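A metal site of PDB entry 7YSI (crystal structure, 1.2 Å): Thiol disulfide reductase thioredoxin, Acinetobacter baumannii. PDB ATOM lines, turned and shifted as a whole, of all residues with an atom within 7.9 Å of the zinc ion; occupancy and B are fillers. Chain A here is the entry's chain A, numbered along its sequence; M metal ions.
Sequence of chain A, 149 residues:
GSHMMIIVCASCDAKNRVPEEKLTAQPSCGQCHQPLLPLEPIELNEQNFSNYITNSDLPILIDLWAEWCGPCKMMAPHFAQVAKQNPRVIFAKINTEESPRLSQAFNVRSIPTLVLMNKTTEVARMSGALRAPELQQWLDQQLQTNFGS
SG of Cys 12 binds the zinc ion, 2.3 Å away.
The side-chain sulfur (SG) of Cys 32 is bound to the zinc ion (2.3 Å).
The zinc ion is bound by SG of Cys 29, 2.3 Å away.
The side-chain sulfur (SG) of Cys 9 binds the zinc ion (2.4 Å).
SG of Cys 12 lies close to N of Ala 14, 3.5 Å away.
The side-chain amide nitrogen of Gln 31 sits close to the side-chain sulfur of Cys 12, 3.6 Å away.
N of Gln 34 lies close to SG of Cys 32.
The backbone NH (N) of Gln 31 lies close to the side-chain sulfur (SG) of Cys 29 (3.4 Å).
N of Cys 29 sits at hydrogen-bond distance from O of Gln 34 (2.8 Å).
The side-chain sulfur of Cys 29 lies close to the side-chain amide nitrogen of Asn 16, 3.6 Å away.
N of Cys 9 sits at hydrogen-bond distance from O of Ala 14 (2.9 Å).
SG of Cys 9 lies close to N of Ser 11 (3.4 Å).
The nearest printed residue that does not touch the zinc ion is Ala 14 (4.5 Å).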
ATOM      1  N   VAL A   8     -15.026   7.032 -18.428  1.00  0.00           N
ATOM      2  CA  VAL A   8     -16.383   6.590 -18.120  1.00  0.00           C
ATOM      3  C   VAL A   8     -16.442   6.124 -16.683  1.00  0.00           C
ATOM      4  O   VAL A   8     -15.501   5.506 -16.196  1.00  0.00           O
ATOM      5  CB  VAL A   8     -16.853   5.481 -19.088  1.00  0.00           C
ATOM      6  CG1 VAL A   8     -18.280   5.042 -18.809  1.00  0.00           C
ATOM      7  CG2 VAL A   8     -16.765   5.933 -20.517  1.00  0.00           C
ATOM      8  N   CYS A   9     -17.560   6.397 -16.018  1.00  0.00           N
ATOM      9  CA  CYS A   9     -17.831   5.838 -14.701  1.00  0.00           C
ATOM     10  C   CYS A   9     -18.597   4.529 -14.870  1.00  0.00           C
ATOM     11  O   CYS A   9     -19.717   4.517 -15.410  1.00  0.00           O
ATOM     12  CB  CYS A   9     -18.680   6.814 -13.901  1.00  0.00           C
ATOM     13  SG  CYS A   9     -19.113   6.179 -12.260  1.00  0.00           S
ATOM     14  N   ALA A  10     -18.031   3.430 -14.382  1.00  0.00           N
ATOM     15  CA  ALA A  10     -18.693   2.136 -14.499  1.00  0.00           C
ATOM     16  C   ALA A  10     -19.894   1.981 -13.553  1.00  0.00           C
ATOM     17  O   ALA A  10     -20.725   1.072 -13.754  1.00  0.00           O
ATOM     18  CB  ALA A  10     -17.678   1.020 -14.198  1.00  0.00           C
ATOM     19  N   SER A  11     -20.002   2.860 -12.560  1.00  0.00           N
ATOM     20  CA  SER A  11     -21.050   2.781 -11.542  1.00  0.00           C
ATOM     21  C   SER A  11     -22.329   3.485 -11.978  1.00  0.00           C
ATOM     22  O   SER A  11     -23.441   2.983 -11.679  1.00  0.00           O
ATOM     23  CB  SER A  11     -20.545   3.410 -10.250  1.00  0.00           C
ATOM     24  OG  SER A  11     -21.399   3.064  -9.167  1.00  0.00           O
ATOM     25  N   CYS A  12     -22.242   4.645 -12.624  1.00  0.00           N
ATOM     26  CA  CYS A  12     -23.418   5.376 -13.053  1.00  0.00           C
ATOM     27  C   CYS A  12     -23.474   5.651 -14.554  1.00  0.00           C
ATOM     28  O   CYS A  12     -24.447   6.268 -15.015  1.00  0.00           O
ATOM     29  CB  CYS A  12     -23.558   6.714 -12.319  1.00  0.00           C
ATOM     30  SG  CYS A  12     -22.489   8.042 -12.953  1.00  0.00           S
ATOM     31  N   ASP A  13     -22.453   5.257 -15.321  1.00  0.00           N
ATOM     32  CA  ASP A  13     -22.339   5.391 -16.780  1.00  0.00           C
ATOM     33  C   ASP A  13     -21.939   6.778 -17.269  1.00  0.00           C
ATOM     34  O   ASP A  13     -21.798   6.965 -18.485  1.00  0.00           O
ATOM     35  CB  ASP A  13     -23.598   4.929 -17.511  1.00  0.00           C
ATOM     36  CG  ASP A  13     -24.058   3.567 -17.048  1.00  0.00           C
ATOM     37  OD1 ASP A  13     -23.220   2.657 -16.957  1.00  0.00           O
ATOM     38  OD2 ASP A  13     -25.251   3.415 -16.684  1.00  0.00           O
ATOM     39  N   ALA A  14     -21.734   7.748 -16.381  1.00  0.00           N
ATOM     40  CA  ALA A  14     -21.425   9.095 -16.836  1.00  0.00           C
ATOM     41  C   ALA A  14     -20.106   9.108 -17.617  1.00  0.00           C
ATOM     42  O   ALA A  14     -19.108   8.498 -17.224  1.00  0.00           O
ATOM     43  CB  ALA A  14     -21.286  10.021 -15.626  1.00  0.00           C
ATOM     44  N   LYS A  15     -20.110   9.848 -18.707  1.00  0.00           N
ATOM     45  CA  LYS A  15     -18.919  10.069 -19.521  1.00  0.00           C
ATOM     46  C   LYS A  15     -18.263  11.339 -18.982  1.00  0.00           C
ATOM     47  O   LYS A  15     -18.675  12.450 -19.324  1.00  0.00           O
ATOM     48  CB  LYS A  15     -19.312  10.267 -20.988  1.00  0.00           C
ATOM     49  CG  LYS A  15     -19.659   8.971 -21.730  1.00  0.00           C
ATOM     50  CD  LYS A  15     -20.641   8.092 -21.051  1.00  0.00           C
ATOM     51  CE  LYS A  15     -22.039   8.484 -21.473  1.00  0.00           C
ATOM     52  NZ  LYS A  15     -23.032   7.520 -20.919  1.00  0.00           N
ATOM     53  N   ASN A  16     -17.266  11.200 -18.119  1.00  0.00           N
ATOM     54  CA  ASN A  16     -16.615  12.360 -17.525  1.00  0.00           C
ATOM     55  C   ASN A  16     -15.579  12.906 -18.495  1.00  0.00           C
ATOM     56  O   ASN A  16     -14.777  12.158 -19.056  1.00  0.00           O
ATOM     57  CB  ASN A  16     -15.898  11.947 -16.234  1.00  0.00           C
ATOM     58  CG  ASN A  16     -16.853  11.757 -15.084  1.00  0.00           C
ATOM     59  OD1 ASN A  16     -16.853  12.542 -14.142  1.00  0.00           O
ATOM     60  ND2 ASN A  16     -17.678  10.737 -15.160  1.00  0.00           N
ATOM     61  N   SER A  28     -12.834  11.815  -8.887  1.00  0.00           N
ATOM     62  CA  SER A  28     -14.073  11.064  -8.750  1.00  0.00           C
ATOM     63  C   SER A  28     -15.073  11.516  -9.804  1.00  0.00           C
ATOM     64  O   SER A  28     -14.994  12.606 -10.340  1.00  0.00           O
ATOM     65  CB  SER A  28     -14.698  11.299  -7.365  1.00  0.00           C
ATOM     66  OG  SER A  28     -13.759  11.049  -6.323  1.00  0.00           O
ATOM     67  N   CYS A  29     -16.022  10.629 -10.083  1.00  0.00           N
ATOM     68  CA  CYS A  29     -17.076  10.914 -11.050  1.00  0.00           C
ATOM     69  C   CYS A  29     -17.830  12.171 -10.669  1.00  0.00           C
ATOM     70  O   CYS A  29     -18.215  12.356  -9.511  1.00  0.00           O
ATOM     71  CB  CYS A  29     -18.059   9.723 -11.103  1.00  0.00           C
ATOM     72  SG  CYS A  29     -19.491   9.954 -12.169  1.00  0.00           S
ATOM     73  N   GLY A  30     -18.059  13.049 -11.656  1.00  0.00           N
ATOM     74  CA  GLY A  30     -18.783  14.287 -11.390  1.00  0.00           C
ATOM     75  C   GLY A  30     -20.252  14.097 -11.074  1.00  0.00           C
ATOM     76  O   GLY A  30     -20.867  15.004 -10.487  1.00  0.00           O
ATOM     77  N   GLN A  31     -20.829  12.950 -11.435  1.00  0.00           N
ATOM     78  CA  GLN A  31     -22.227  12.674 -11.134  1.00  0.00           C
ATOM     79  C   GLN A  31     -22.358  11.961  -9.777  1.00  0.00           C
ATOM     80  O   GLN A  31     -23.020  12.476  -8.869  1.00  0.00           O
ATOM     81  CB  GLN A  31     -22.866  11.824 -12.231  1.00  0.00           C
ATOM     82  CG  GLN A  31     -24.338  11.476 -12.006  1.00  0.00           C
ATOM     83  CD  GLN A  31     -24.937  10.542 -13.082  1.00  0.00           C
ATOM     84  OE1 GLN A  31     -24.705  10.732 -14.272  1.00  0.00           O
ATOM     85  NE2 GLN A  31     -25.722   9.559 -12.654  1.00  0.00           N
ATOM     86  N   CYS A  32     -21.727  10.796  -9.617  1.00  0.00           N
ATOM     87  CA  CYS A  32     -21.963   9.950  -8.452  1.00  0.00           C
ATOM     88  C   CYS A  32     -20.817   9.914  -7.461  1.00  0.00           C
ATOM     89  O   CYS A  32     -20.959   9.297  -6.392  1.00  0.00           O
ATOM     90  CB  CYS A  32     -22.310   8.521  -8.876  1.00  0.00           C
ATOM     91  SG  CYS A  32     -20.873   7.555  -9.417  1.00  0.00           S
ATOM     92  N   HIS A  33     -19.686  10.527  -7.777  1.00  0.00           N
ATOM     93  CA  HIS A  33     -18.528  10.647  -6.904  1.00  0.00           C
ATOM     94  C   HIS A  33     -17.794   9.338  -6.628  1.00  0.00           C
ATOM     95  O   HIS A  33     -16.936   9.305  -5.733  1.00  0.00           O
ATOM     96  CB  HIS A  33     -18.843  11.340  -5.566  1.00  0.00           C
ATOM     97  CG  HIS A  33     -19.438  12.702  -5.712  1.00  0.00           C
ATOM     98  ND1 HIS A  33     -20.013  13.372  -4.645  1.00  0.00           N
ATOM     99  CD2 HIS A  33     -19.563  13.520  -6.788  1.00  0.00           C
ATOM    100  CE1 HIS A  33     -20.472  14.531  -5.072  1.00  0.00           C
ATOM    101  NE2 HIS A  33     -20.203  14.655  -6.358  1.00  0.00           N
ATOM    102  N   GLN A  34     -18.061   8.265  -7.369  1.00  0.00           N
ATOM    103  CA  GLN A  34     -17.219   7.087  -7.275  1.00  0.00           C
ATOM    104  C   GLN A  34     -15.864   7.329  -7.966  1.00  0.00           C
ATOM    105  O   GLN A  34     -15.745   8.163  -8.869  1.00  0.00           O
ATOM    106  CB  GLN A  34     -17.902   5.867  -7.913  1.00  0.00           C
ATOM    107  CG  GLN A  34     -19.082   5.345  -7.089  1.00  0.00           C
ATOM    108  CD  GLN A  34     -18.641   4.942  -5.689  1.00  0.00           C
ATOM    109  OE1 GLN A  34     -17.766   4.096  -5.526  1.00  0.00           O
ATOM    110  NE2 GLN A  34     -19.222   5.576  -4.687  1.00  0.00           N
ATOM    111  N   PRO A  35     -14.809   6.622  -7.541  1.00  0.00           N
ATOM    112  CA  PRO A  35     -13.485   6.854  -8.152  1.00  0.00           C
ATOM    113  C   PRO A  35     -13.478   6.522  -9.638  1.00  0.00           C
ATOM    114  O   PRO A  35     -13.937   5.466 -10.060  1.00  0.00           O
ATOM    115  CB  PRO A  35     -12.549   5.922  -7.348  1.00  0.00           C
ATOM    116  CG  PRO A  35     -13.288   5.655  -6.023  1.00  0.00           C
ATOM    117  CD  PRO A  35     -14.745   5.612  -6.456  1.00  0.00           C
ATOM    118  N   LEU A  36     -12.910   7.408 -10.444  1.00  0.00           N
ATOM    119  CA  LEU A  36     -12.827   7.148 -11.886  1.00  0.00           C
ATOM    120  C   LEU A  36     -11.613   6.340 -12.267  1.00  0.00           C
ATOM    121  O   LEU A  36     -11.645   5.578 -13.239  1.00  0.00           O
ATOM    122  CB  LEU A  36     -12.780   8.466 -12.673  1.00  0.00           C
ATOM    123  CG  LEU A  36     -14.067   9.266 -12.703  1.00  0.00           C
ATOM    124  CD1 LEU A  36     -13.782  10.624 -13.312  1.00  0.00           C
ATOM    125  CD2 LEU A  36     -15.117   8.532 -13.495  1.00  0.00           C
HETATM  126 ZN    ZN M   1     -20.578   7.948 -11.688  1.00  0.00          ZN
